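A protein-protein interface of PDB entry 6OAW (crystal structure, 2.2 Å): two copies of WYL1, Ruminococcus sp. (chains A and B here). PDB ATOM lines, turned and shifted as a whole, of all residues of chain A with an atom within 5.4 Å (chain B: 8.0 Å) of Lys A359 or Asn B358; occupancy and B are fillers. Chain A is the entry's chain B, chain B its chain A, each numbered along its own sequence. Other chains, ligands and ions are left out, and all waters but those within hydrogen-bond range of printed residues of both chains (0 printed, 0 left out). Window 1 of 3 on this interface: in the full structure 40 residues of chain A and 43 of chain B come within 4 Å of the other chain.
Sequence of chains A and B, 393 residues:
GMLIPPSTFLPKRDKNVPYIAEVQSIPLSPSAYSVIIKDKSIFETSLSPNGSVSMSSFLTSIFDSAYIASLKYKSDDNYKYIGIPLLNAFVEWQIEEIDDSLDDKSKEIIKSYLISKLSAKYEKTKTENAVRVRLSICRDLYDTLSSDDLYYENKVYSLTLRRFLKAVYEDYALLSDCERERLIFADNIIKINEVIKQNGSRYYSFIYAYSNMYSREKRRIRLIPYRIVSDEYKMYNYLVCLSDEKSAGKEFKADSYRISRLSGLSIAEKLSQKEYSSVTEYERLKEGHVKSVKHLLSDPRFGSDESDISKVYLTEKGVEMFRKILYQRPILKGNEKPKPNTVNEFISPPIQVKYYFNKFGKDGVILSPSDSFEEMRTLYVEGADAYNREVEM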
ATOM      1  N   MET A 321      -1.244  -1.665 -14.130  1.00  0.00           N
ATOM      2  CA  MET A 321      -0.541  -2.545 -15.113  1.00  0.00           C
ATOM      3  C   MET A 321      -1.600  -3.081 -16.083  1.00  0.00           C
ATOM      4  O   MET A 321      -1.354  -3.173 -17.305  1.00  0.00           O
ATOM      5  CB  MET A 321       0.211  -3.671 -14.397  1.00  0.00           C
ATOM      6  CG  MET A 321       1.472  -3.212 -13.672  1.00  0.00           C
ATOM      7  SD  MET A 321       2.212  -4.636 -12.497  1.00  0.00           S
ATOM      8  CE  MET A 321       2.646  -6.105 -13.725  1.00  0.00           C
ATOM      9  N   ILE A 325      -1.243  -2.748 -20.129  1.00  0.00           N
ATOM     10  CA  ILE A 325      -0.846  -3.979 -20.872  1.00  0.00           C
ATOM     11  C   ILE A 325      -2.105  -4.617 -21.476  1.00  0.00           C
ATOM     12  O   ILE A 325      -2.893  -5.282 -20.755  1.00  0.00           O
ATOM     13  CB  ILE A 325      -0.043  -4.919 -19.940  1.00  0.00           C
ATOM     14  CG1 ILE A 325       1.199  -4.226 -19.364  1.00  0.00           C
ATOM     15  CG2 ILE A 325       0.327  -6.229 -20.629  1.00  0.00           C
ATOM     16  CD1 ILE A 325       1.843  -5.005 -18.259  1.00  0.00           C
ATOM     17  N   LYS A 354      -4.221 -16.896 -16.791  1.00  0.00           N
ATOM     18  CA  LYS A 354      -2.898 -17.404 -16.347  1.00  0.00           C
ATOM     19  C   LYS A 354      -1.780 -16.772 -17.204  1.00  0.00           C
ATOM     20  O   LYS A 354      -0.791 -16.234 -16.646  1.00  0.00           O
ATOM     21  CB  LYS A 354      -2.915 -18.918 -16.562  1.00  0.00           C
ATOM     22  CG  LYS A 354      -2.346 -19.804 -15.494  1.00  0.00           C
ATOM     23  CD  LYS A 354      -1.549 -20.946 -16.068  1.00  0.00           C
ATOM     24  CE  LYS A 354      -2.353 -21.925 -16.888  1.00  0.00           C
ATOM     25  NZ  LYS A 354      -1.482 -22.620 -17.862  1.00  0.00           N
ATOM     26  N   TYR A 355      -1.915 -16.809 -18.534  1.00  0.00           N
ATOM     27  CA  TYR A 355      -0.902 -16.227 -19.457  1.00  0.00           C
ATOM     28  C   TYR A 355      -0.834 -14.709 -19.253  1.00  0.00           C
ATOM     29  O   TYR A 355       0.212 -14.126 -19.521  1.00  0.00           O
ATOM     30  CB  TYR A 355      -1.142 -16.537 -20.941  1.00  0.00           C
ATOM     31  CG  TYR A 355      -0.997 -17.976 -21.360  1.00  0.00           C
ATOM     32  CD1 TYR A 355      -0.311 -18.894 -20.583  1.00  0.00           C
ATOM     33  CD2 TYR A 355      -1.502 -18.409 -22.571  1.00  0.00           C
ATOM     34  CE1 TYR A 355      -0.141 -20.206 -20.999  1.00  0.00           C
ATOM     35  CE2 TYR A 355      -1.359 -19.717 -22.994  1.00  0.00           C
ATOM     36  CZ  TYR A 355      -0.674 -20.616 -22.204  1.00  0.00           C
ATOM     37  OH  TYR A 355      -0.503 -21.901 -22.634  1.00  0.00           O
ATOM     38  N   TYR A 356      -1.874 -14.072 -18.717  1.00  0.00           N
ATOM     39  CA  TYR A 356      -1.825 -12.608 -18.496  1.00  0.00           C
ATOM     40  C   TYR A 356      -1.182 -12.257 -17.152  1.00  0.00           C
ATOM     41  O   TYR A 356      -0.349 -11.329 -17.093  1.00  0.00           O
ATOM     42  CB  TYR A 356      -3.209 -11.992 -18.543  1.00  0.00           C
ATOM     43  CG  TYR A 356      -3.177 -10.496 -18.527  1.00  0.00           C
ATOM     44  CD1 TYR A 356      -2.743  -9.777 -19.624  1.00  0.00           C
ATOM     45  CD2 TYR A 356      -3.510  -9.788 -17.384  1.00  0.00           C
ATOM     46  CE1 TYR A 356      -2.718  -8.395 -19.607  1.00  0.00           C
ATOM     47  CE2 TYR A 356      -3.453  -8.406 -17.344  1.00  0.00           C
ATOM     48  CZ  TYR A 356      -3.075  -7.704 -18.466  1.00  0.00           C
ATOM     49  OH  TYR A 356      -3.039  -6.333 -18.449  1.00  0.00           O
ATOM     50  N   PHE A 357      -1.597 -12.947 -16.084  1.00  0.00           N
ATOM     51  CA  PHE A 357      -1.211 -12.568 -14.709  1.00  0.00           C
ATOM     52  C   PHE A 357       0.053 -13.316 -14.255  1.00  0.00           C
ATOM     53  O   PHE A 357       0.538 -12.993 -13.169  1.00  0.00           O
ATOM     54  CB  PHE A 357      -2.396 -12.726 -13.777  1.00  0.00           C
ATOM     55  CG  PHE A 357      -3.468 -11.700 -13.992  1.00  0.00           C
ATOM     56  CD1 PHE A 357      -3.221 -10.369 -13.721  1.00  0.00           C
ATOM     57  CD2 PHE A 357      -4.731 -12.073 -14.435  1.00  0.00           C
ATOM     58  CE1 PHE A 357      -4.232  -9.436 -13.891  1.00  0.00           C
ATOM     59  CE2 PHE A 357      -5.722 -11.130 -14.636  1.00  0.00           C
ATOM     60  CZ  PHE A 357      -5.477  -9.817 -14.347  1.00  0.00           C
ATOM     61  N   ASN A 358       0.599 -14.234 -15.054  1.00  0.00           N
ATOM     62  CA  ASN A 358       1.844 -14.942 -14.663  1.00  0.00           C
ATOM     63  C   ASN A 358       3.001 -13.952 -14.445  1.00  0.00           C
ATOM     64  O   ASN A 358       3.899 -14.309 -13.674  1.00  0.00           O
ATOM     65  CB  ASN A 358       2.229 -16.058 -15.636  1.00  0.00           C
ATOM     66  CG  ASN A 358       2.480 -15.603 -17.057  1.00  0.00           C
ATOM     67  OD1 ASN A 358       2.536 -14.401 -17.317  1.00  0.00           O
ATOM     68  ND2 ASN A 358       2.661 -16.568 -17.948  1.00  0.00           N
ATOM     69  N   LYS A 359       2.986 -12.755 -15.056  1.00  0.00           N
ATOM     70  CA  LYS A 359       4.048 -11.737 -14.856  1.00  0.00           C
ATOM     71  C   LYS A 359       3.685 -10.715 -13.775  1.00  0.00           C
ATOM     72  O   LYS A 359       4.445  -9.805 -13.569  1.00  0.00           O
ATOM     73  CB  LYS A 359       4.361 -11.018 -16.163  1.00  0.00           C
ATOM     74  CG  LYS A 359       3.162 -10.345 -16.826  1.00  0.00           C
ATOM     75  CD  LYS A 359       3.494  -9.580 -18.037  1.00  0.00           C
ATOM     76  CE  LYS A 359       2.250  -9.164 -18.770  1.00  0.00           C
ATOM     77  NZ  LYS A 359       1.442 -10.347 -19.130  1.00  0.00           N
ATOM     78  N   PHE A 360       2.587 -10.850 -13.048  1.00  0.00           N
ATOM     79  CA  PHE A 360       2.131  -9.781 -12.118  1.00  0.00           C
ATOM     80  C   PHE A 360       2.633 -10.006 -10.694  1.00  0.00           C
ATOM     81  O   PHE A 360       2.561  -9.069  -9.936  1.00  0.00           O
ATOM     82  CB  PHE A 360       0.611  -9.710 -12.114  1.00  0.00           C
ATOM     83  CG  PHE A 360       0.016  -8.793 -13.142  1.00  0.00           C
ATOM     84  CD1 PHE A 360       0.149  -9.054 -14.498  1.00  0.00           C
ATOM     85  CD2 PHE A 360      -0.728  -7.692 -12.749  1.00  0.00           C
ATOM     86  CE1 PHE A 360      -0.441  -8.216 -15.434  1.00  0.00           C
ATOM     87  CE2 PHE A 360      -1.278  -6.844 -13.689  1.00  0.00           C
ATOM     88  CZ  PHE A 360      -1.140  -7.109 -15.029  1.00  0.00           C
ATOM     89  N   GLY A 361       3.051 -11.223 -10.334  1.00  0.00           N
ATOM     90  CA  GLY A 361       3.407 -11.575  -8.955  1.00  0.00           C
ATOM     91  C   GLY A 361       2.341 -11.123  -7.977  1.00  0.00           C
ATOM     92  O   GLY A 361       1.185 -11.441  -8.208  1.00  0.00           O
ATOM     93  N   TYR A 380       6.327 -19.233  -9.092  1.00  0.00           N
ATOM     94  CA  TYR A 380       6.883 -18.153  -8.244  1.00  0.00           C
ATOM     95  C   TYR A 380       7.802 -18.754  -7.189  1.00  0.00           C
ATOM     96  O   TYR A 380       8.869 -18.159  -6.986  1.00  0.00           O
ATOM     97  CB  TYR A 380       5.777 -17.275  -7.657  1.00  0.00           C
ATOM     98  CG  TYR A 380       5.438 -16.175  -8.615  1.00  0.00           C
ATOM     99  CD1 TYR A 380       6.198 -15.021  -8.652  1.00  0.00           C
ATOM    100  CD2 TYR A 380       4.488 -16.364  -9.597  1.00  0.00           C
ATOM    101  CE1 TYR A 380       5.993 -14.050  -9.614  1.00  0.00           C
ATOM    102  CE2 TYR A 380       4.278 -15.402 -10.569  1.00  0.00           C
ATOM    103  CZ  TYR A 380       5.023 -14.231 -10.569  1.00  0.00           C
ATOM    104  OH  TYR A 380       4.818 -13.250 -11.504  1.00  0.00           O
ATOM    105  N   MET B 321      10.508 -23.435 -24.285  1.00  0.00           N
ATOM    106  CA  MET B 321       9.511 -22.341 -24.149  1.00  0.00           C
ATOM    107  C   MET B 321       9.939 -21.212 -25.105  1.00  0.00           C
ATOM    108  O   MET B 321       9.080 -20.601 -25.765  1.00  0.00           O
ATOM    109  CB  MET B 321       9.432 -21.863 -22.693  1.00  0.00           C
ATOM    110  CG  MET B 321       8.727 -22.838 -21.740  1.00  0.00           C
ATOM    111  SD  MET B 321       8.984 -22.260 -19.867  1.00  0.00           S
ATOM    112  CE  MET B 321       8.103 -20.485 -19.768  1.00  0.00           C
ATOM    113  N   TYR B 327       6.290 -14.114 -29.308  1.00  0.00           N
ATOM    114  CA  TYR B 327       5.865 -12.721 -29.046  1.00  0.00           C
ATOM    115  C   TYR B 327       6.980 -11.914 -28.380  1.00  0.00           C
ATOM    116  O   TYR B 327       7.371 -12.239 -27.298  1.00  0.00           O
ATOM    117  CB  TYR B 327       4.617 -12.681 -28.173  1.00  0.00           C
ATOM    118  CG  TYR B 327       4.075 -11.289 -28.055  1.00  0.00           C
ATOM    119  CD1 TYR B 327       3.720 -10.584 -29.191  1.00  0.00           C
ATOM    120  CD2 TYR B 327       3.977 -10.660 -26.826  1.00  0.00           C
ATOM    121  CE1 TYR B 327       3.273  -9.280 -29.107  1.00  0.00           C
ATOM    122  CE2 TYR B 327       3.478  -9.365 -26.728  1.00  0.00           C
ATOM    123  CZ  TYR B 327       3.119  -8.683 -27.865  1.00  0.00           C
ATOM    124  OH  TYR B 327       2.646  -7.405 -27.810  1.00  0.00           O
ATOM    125  N   ILE B 351      15.040  -4.037 -21.415  1.00  0.00           N
ATOM    126  CA  ILE B 351      13.573  -3.953 -21.142  1.00  0.00           C
ATOM    127  C   ILE B 351      12.838  -5.106 -21.835  1.00  0.00           C
ATOM    128  O   ILE B 351      11.956  -5.707 -21.194  1.00  0.00           O
ATOM    129  CB  ILE B 351      12.990  -2.586 -21.531  1.00  0.00           C
ATOM    130  CG1 ILE B 351      13.374  -1.554 -20.480  1.00  0.00           C
ATOM    131  CG2 ILE B 351      11.471  -2.689 -21.692  1.00  0.00           C
ATOM    132  CD1 ILE B 351      12.528  -0.298 -20.518  1.00  0.00           C
ATOM    133  N   GLN B 352      13.189  -5.410 -23.085  1.00  0.00           N
ATOM    134  CA  GLN B 352      12.507  -6.458 -23.890  1.00  0.00           C
ATOM    135  C   GLN B 352      12.874  -7.834 -23.341  1.00  0.00           C
ATOM    136  O   GLN B 352      11.985  -8.670 -23.254  1.00  0.00           O
ATOM    137  CB  GLN B 352      12.878  -6.358 -25.360  1.00  0.00           C
ATOM    138  CG  GLN B 352      12.117  -7.327 -26.251  1.00  0.00           C
ATOM    139  CD  GLN B 352      12.625  -7.221 -27.669  1.00  0.00           C
ATOM    140  OE1 GLN B 352      13.126  -6.168 -28.101  1.00  0.00           O
ATOM    141  NE2 GLN B 352      12.458  -8.295 -28.425  1.00  0.00           N
ATOM    142  N   VAL B 353      14.126  -8.033 -22.913  1.00  0.00           N
ATOM    143  CA  VAL B 353      14.548  -9.319 -22.292  1.00  0.00           C
ATOM    144  C   VAL B 353      13.664  -9.546 -21.053  1.00  0.00           C
ATOM    145  O   VAL B 353      13.122 -10.646 -20.890  1.00  0.00           O
ATOM    146  CB  VAL B 353      16.046  -9.336 -21.932  1.00  0.00           C
ATOM    147  CG1 VAL B 353      16.488 -10.710 -21.453  1.00  0.00           C
ATOM    148  CG2 VAL B 353      16.898  -8.893 -23.111  1.00  0.00           C
ATOM    149  N   LYS B 354      13.567  -8.530 -20.202  1.00  0.00           N
ATOM    150  CA  LYS B 354      12.809  -8.540 -18.932  1.00  0.00           C
ATOM    151  C   LYS B 354      11.314  -8.806 -19.225  1.00  0.00           C
ATOM    152  O   LYS B 354      10.743  -9.672 -18.568  1.00  0.00           O
ATOM    153  CB  LYS B 354      13.165  -7.207 -18.286  1.00  0.00           C
ATOM    154  CG  LYS B 354      12.611  -6.889 -16.912  1.00  0.00           C
ATOM    155  CD  LYS B 354      13.313  -5.677 -16.344  1.00  0.00           C
ATOM    156  CE  LYS B 354      12.922  -4.382 -17.041  1.00  0.00           C
ATOM    157  NZ  LYS B 354      13.905  -3.311 -16.790  1.00  0.00           N
ATOM    158  N   TYR B 355      10.709  -8.132 -20.217  1.00  0.00           N
ATOM    159  CA  TYR B 355       9.285  -8.342 -20.591  1.00  0.00           C
ATOM    160  C   TYR B 355       9.113  -9.746 -21.185  1.00  0.00           C
ATOM    161  O   TYR B 355       8.010 -10.257 -21.148  1.00  0.00           O
ATOM    162  CB  TYR B 355       8.739  -7.283 -21.563  1.00  0.00           C
ATOM    163  CG  TYR B 355       8.574  -5.880 -21.022  1.00  0.00           C
ATOM    164  CD1 TYR B 355       8.728  -5.598 -19.673  1.00  0.00           C
ATOM    165  CD2 TYR B 355       8.256  -4.823 -21.866  1.00  0.00           C
ATOM    166  CE1 TYR B 355       8.604  -4.310 -19.181  1.00  0.00           C
ATOM    167  CE2 TYR B 355       8.109  -3.525 -21.392  1.00  0.00           C
ATOM    168  CZ  TYR B 355       8.292  -3.273 -20.041  1.00  0.00           C
ATOM    169  OH  TYR B 355       8.157  -2.027 -19.499  1.00  0.00           O
ATOM    170  N   TYR B 356      10.164 -10.405 -21.648  1.00  0.00           N
ATOM    171  CA  TYR B 356      10.014 -11.775 -22.201  1.00  0.00           C
ATOM    172  C   TYR B 356      10.187 -12.831 -21.101  1.00  0.00           C
ATOM    173  O   TYR B 356       9.413 -13.836 -21.095  1.00  0.00           O
ATOM    174  CB  TYR B 356      11.061 -12.089 -23.261  1.00  0.00           C
ATOM    175  CG  TYR B 356      10.833 -13.403 -23.956  1.00  0.00           C
ATOM    176  CD1 TYR B 356       9.824 -13.549 -24.881  1.00  0.00           C
ATOM    177  CD2 TYR B 356      11.635 -14.490 -23.701  1.00  0.00           C
ATOM    178  CE1 TYR B 356       9.640 -14.740 -25.557  1.00  0.00           C
ATOM    179  CE2 TYR B 356      11.458 -15.695 -24.356  1.00  0.00           C
ATOM    180  CZ  TYR B 356      10.449 -15.829 -25.286  1.00  0.00           C
ATOM    181  OH  TYR B 356      10.290 -17.019 -25.962  1.00  0.00           O
ATOM    182  N   PHE B 357      11.208 -12.677 -20.260  1.00  0.00           N
ATOM    183  CA  PHE B 357      11.621 -13.748 -19.316  1.00  0.00           C
ATOM    184  C   PHE B 357      10.966 -13.529 -17.948  1.00  0.00           C
ATOM    185  O   PHE B 357      11.117 -14.413 -17.065  1.00  0.00           O
ATOM    186  CB  PHE B 357      13.147 -13.865 -19.225  1.00  0.00           C
ATOM    187  CG  PHE B 357      13.771 -14.477 -20.453  1.00  0.00           C
ATOM    188  CD1 PHE B 357      13.536 -15.797 -20.781  1.00  0.00           C
ATOM    189  CD2 PHE B 357      14.607 -13.743 -21.282  1.00  0.00           C
ATOM    190  CE1 PHE B 357      14.126 -16.369 -21.896  1.00  0.00           C
ATOM    191  CE2 PHE B 357      15.188 -14.312 -22.404  1.00  0.00           C
ATOM    192  CZ  PHE B 357      14.950 -15.621 -22.719  1.00  0.00           C
ATOM    193  N   ASN B 358      10.195 -12.457 -17.765  1.00  0.00           N
ATOM    194  CA  ASN B 358       9.498 -12.243 -16.465  1.00  0.00           C
ATOM    195  C   ASN B 358       8.538 -13.412 -16.168  1.00  0.00           C
ATOM    196  O   ASN B 358       8.281 -13.624 -15.008  1.00  0.00           O
ATOM    197  CB  ASN B 358       8.816 -10.877 -16.382  1.00  0.00           C
ATOM    198  CG  ASN B 358       7.755 -10.648 -17.438  1.00  0.00           C
ATOM    199  OD1 ASN B 358       7.417 -11.553 -18.218  1.00  0.00           O
ATOM    200  ND2 ASN B 358       7.219  -9.429 -17.460  1.00  0.00           N
ATOM    201  N   LYS B 359       8.025 -14.133 -17.175  1.00  0.00           N
ATOM    202  CA  LYS B 359       7.102 -15.280 -16.994  1.00  0.00           C
ATOM    203  C   LYS B 359       7.850 -16.625 -16.984  1.00  0.00           C
ATOM    204  O   LYS B 359       7.190 -17.619 -16.883  1.00  0.00           O
ATOM    205  CB  LYS B 359       6.034 -15.280 -18.084  1.00  0.00           C
ATOM    206  CG  LYS B 359       6.572 -15.336 -19.505  1.00  0.00           C
ATOM    207  CD  LYS B 359       5.524 -15.561 -20.557  1.00  0.00           C
ATOM    208  CE  LYS B 359       6.014 -15.234 -21.944  1.00  0.00           C
ATOM    209  NZ  LYS B 359       6.578 -13.857 -21.981  1.00  0.00           N
ATOM    210  N   PHE B 360       9.184 -16.682 -17.008  1.00  0.00           N
ATOM    211  CA  PHE B 360       9.920 -17.965 -17.163  1.00  0.00           C
ATOM    212  C   PHE B 360      10.287 -18.598 -15.817  1.00  0.00           C
ATOM    213  O   PHE B 360      10.567 -19.834 -15.804  1.00  0.00           O
ATOM    214  CB  PHE B 360      11.197 -17.765 -17.968  1.00  0.00           C
ATOM    215  CG  PHE B 360      11.017 -17.985 -19.443  1.00  0.00           C
ATOM    216  CD1 PHE B 360      10.205 -17.136 -20.180  1.00  0.00           C
ATOM    217  CD2 PHE B 360      11.663 -19.022 -20.088  1.00  0.00           C
ATOM    218  CE1 PHE B 360      10.032 -17.328 -21.538  1.00  0.00           C
ATOM    219  CE2 PHE B 360      11.468 -19.222 -21.450  1.00  0.00           C
ATOM    220  CZ  PHE B 360      10.667 -18.365 -22.169  1.00  0.00           C
ATOM    221  N   GLY B 361      10.340 -17.800 -14.746  1.00  0.00           N
ATOM    222  CA  GLY B 361      10.835 -18.271 -13.451  1.00  0.00           C
ATOM    223  C   GLY B 361      12.196 -18.933 -13.617  1.00  0.00           C
ATOM    224  O   GLY B 361      13.100 -18.357 -14.293  1.00  0.00           O
ATOM    225  N   LYS B 362      12.374 -20.110 -13.023  1.00  0.00           N
ATOM    226  CA  LYS B 362      13.696 -20.764 -12.912  1.00  0.00           C
ATOM    227  C   LYS B 362      14.155 -21.292 -14.276  1.00  0.00           C
ATOM    228  O   LYS B 362      15.320 -21.632 -14.392  1.00  0.00           O
ATOM    229  CB  LYS B 362      13.605 -21.904 -11.898  1.00  0.00           C
ATOM    230  CG  LYS B 362      12.832 -23.110 -12.384  1.00  0.00           C
ATOM    231  CD  LYS B 362      13.312 -24.405 -11.810  1.00  0.00           C
ATOM    232  CE  LYS B 362      12.362 -25.536 -12.122  1.00  0.00           C
ATOM    233  NZ  LYS B 362      12.770 -26.750 -11.395  1.00  0.00           N
ATOM    234  N   GLY B 364      14.187 -19.440 -17.025  1.00  0.00           N
ATOM    235  CA  GLY B 364      14.800 -18.279 -17.724  1.00  0.00           C
ATOM    236  C   GLY B 364      15.206 -17.213 -16.723  1.00  0.00           C
ATOM    237  O   GLY B 364      14.418 -16.314 -16.485  1.00  0.00           O
ATOM    238  N   ILE B 366      17.198 -14.149 -15.409  1.00  0.00           N
ATOM    239  CA  ILE B 366      18.024 -12.995 -15.850  1.00  0.00           C
ATOM    240  C   ILE B 366      19.075 -12.709 -14.787  1.00  0.00           C
ATOM    241  O   ILE B 366      18.696 -12.197 -13.737  1.00  0.00           O
ATOM    242  CB  ILE B 366      17.196 -11.745 -16.194  1.00  0.00           C
ATOM    243  CG1 ILE B 366      16.026 -12.093 -17.119  1.00  0.00           C
ATOM    244  CG2 ILE B 366      18.109 -10.683 -16.803  1.00  0.00           C
ATOM    245  CD1 ILE B 366      15.117 -10.902 -17.455  1.00  0.00           C
ATOM    246  N   GLU B 375      15.093  -6.494 -10.216  1.00  0.00           N
ATOM    247  CA  GLU B 375      13.627  -6.379 -10.469  1.00  0.00           C
ATOM    248  C   GLU B 375      13.013  -7.786 -10.496  1.00  0.00           C
ATOM    249  O   GLU B 375      11.967  -7.978  -9.905  1.00  0.00           O
ATOM    250  CB  GLU B 375      13.321  -5.617 -11.764  1.00  0.00           C
ATOM    251  N   MET B 376      13.636  -8.715 -11.206  1.00  0.00           N
ATOM    252  CA  MET B 376      13.100 -10.084 -11.356  1.00  0.00           C
ATOM    253  C   MET B 376      13.128 -10.758  -9.994  1.00  0.00           C
ATOM    254  O   MET B 376      12.130 -11.391  -9.654  1.00  0.00           O
ATOM    255  CB  MET B 376      13.889 -10.892 -12.388  1.00  0.00           C
ATOM    256  CG  MET B 376      13.741 -10.382 -13.802  1.00  0.00           C
ATOM    257  SD  MET B 376      11.850 -10.361 -14.388  1.00  0.00           S
ATOM    258  CE  MET B 376      11.165  -8.560 -13.919  1.00  0.00           C
ATOM    259  N   LEU B 379      10.218  -9.287  -8.049  1.00  0.00           N
ATOM    260  CA  LEU B 379       8.938  -9.809  -8.612  1.00  0.00           C
ATOM    261  C   LEU B 379       8.697 -11.236  -8.082  1.00  0.00           C
ATOM    262  O   LEU B 379       7.590 -11.518  -7.556  1.00  0.00           O
ATOM    263  CB  LEU B 379       8.988  -9.797 -10.139  1.00  0.00           C
ATOM    264  CG  LEU B 379       7.812 -10.472 -10.851  1.00  0.00           C
ATOM    265  CD1 LEU B 379       6.530  -9.642 -10.691  1.00  0.00           C
ATOM    266  CD2 LEU B 379       8.137 -10.662 -12.329  1.00  0.00           C
ATOM    267  N   TYR B 380       9.708 -12.093  -8.166  1.00  0.00           N
ATOM    268  CA  TYR B 380       9.584 -13.535  -7.829  1.00  0.00           C
ATOM    269  C   TYR B 380       9.480 -13.713  -6.316  1.00  0.00           C
ATOM    270  O   TYR B 380       8.633 -14.498  -5.901  1.00  0.00           O
ATOM    271  CB  TYR B 380      10.684 -14.368  -8.504  1.00  0.00           C
ATOM    272  CG  TYR B 380      10.206 -14.789  -9.861  1.00  0.00           C
ATOM    273  CD1 TYR B 380      10.375 -13.966 -10.965  1.00  0.00           C
ATOM    274  CD2 TYR B 380       9.421 -15.918 -10.005  1.00  0.00           C
ATOM    275  CE1 TYR B 380       9.856 -14.302 -12.206  1.00  0.00           C
ATOM    276  CE2 TYR B 380       8.880 -16.260 -11.237  1.00  0.00           C
ATOM    277  CZ  TYR B 380       9.078 -15.438 -12.337  1.00  0.00           C
ATOM    278  OH  TYR B 380       8.537 -15.776 -13.546  1.00  0.00           O
ATOM    279  N   TYR B 387       1.630 -15.814  -2.996  1.00  0.00           N
ATOM    280  CA  TYR B 387       0.989 -17.135  -3.258  1.00  0.00           C
ATOM    281  C   TYR B 387       1.070 -18.031  -2.009  1.00  0.00           C
ATOM    282  O   TYR B 387       0.056 -18.627  -1.663  1.00  0.00           O
ATOM    283  CB  TYR B 387       1.574 -17.792  -4.509  1.00  0.00           C
ATOM    284  CG  TYR B 387       1.026 -17.200  -5.777  1.00  0.00           C
ATOM    285  CD1 TYR B 387      -0.205 -17.606  -6.264  1.00  0.00           C
ATOM    286  CD2 TYR B 387       1.723 -16.220  -6.470  1.00  0.00           C
ATOM    287  CE1 TYR B 387      -0.761 -17.024  -7.387  1.00  0.00           C
ATOM    288  CE2 TYR B 387       1.192 -15.650  -7.625  1.00  0.00           C
ATOM    289  CZ  TYR B 387      -0.038 -16.083  -8.092  1.00  0.00           C
ATOM    290  OH  TYR B 387      -0.565 -15.547  -9.210  1.00  0.00           O
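The side-chain hydroxyl (OH) of Tyr A380 lies within hydrogen-bond range of the backbone NH (N) of Gly A361 (2.9 Å).
O of Tyr B355 sits close to OD1 of Asn B358, 3.3 Å away.
The backbone carbonyl oxygen (O) of Asn B358 sits at hydrogen-bond distance from the side-chain hydroxyl (OH) of Tyr B380, at 2.6 Å.
The side-chain amide oxygen (OD1) of Asn A358 lies close to the backbone carbonyl oxygen (O) of Tyr A355, at 3.2 Å.
The backbone carbonyl oxygen of Asn A358 sits at hydrogen-bond distance from the side-chain hydroxyl of Tyr A380 (2.6 Å).
The backbone NH (N) of Gly B361 lies within hydrogen-bond range of the side-chain hydroxyl (OH) of Tyr B380, at 3.0 Å.
Asn A358 touches Lys B359 (ND2 to CB, 3.6 Å).
Lys A359 touches Asn B358 (CB to ND2, 3.5 Å).
O of Lys A359 touches CD1 of Leu B379, 3.6 Å away.
C of Phe A360 touches CD1 of Leu B379, at 3.9 Å.
Gly A361 touches Leu B379 (N to CD1, 3.8 Å).
Tyr A380 touches Leu B379.
Tyr A380 touches Tyr B380 (CD1 to CD2, 3.6 Å).
CE2 of Tyr B387 touches CD2 of Tyr A380, at 3.9 Å.
Lys A359 touches just these residues of chain B: Asn B358 and Leu B379.
Printed residues of chain B within 4 Å of Phe A360: Leu B379.
Of the printed residues of chain B, Tyr A380 touches Leu B379 (3.6 Å), Tyr B380 (3.6 Å) and Tyr B387 (3.9 Å).
Asn B358 touches just one residue of chain A: Lys A359.
Lys B362 touches none of the printed residues of chain A.
Of the 21 printed residues of chain B, 5 touch a printed residue of chain A.
Asn A358 touches Lys B359, and with the chains exchanged Lys A359 touches Asn B358.
Tyr B380 touches its own counterpart, Tyr A380.
10 positions are printed for both chains.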
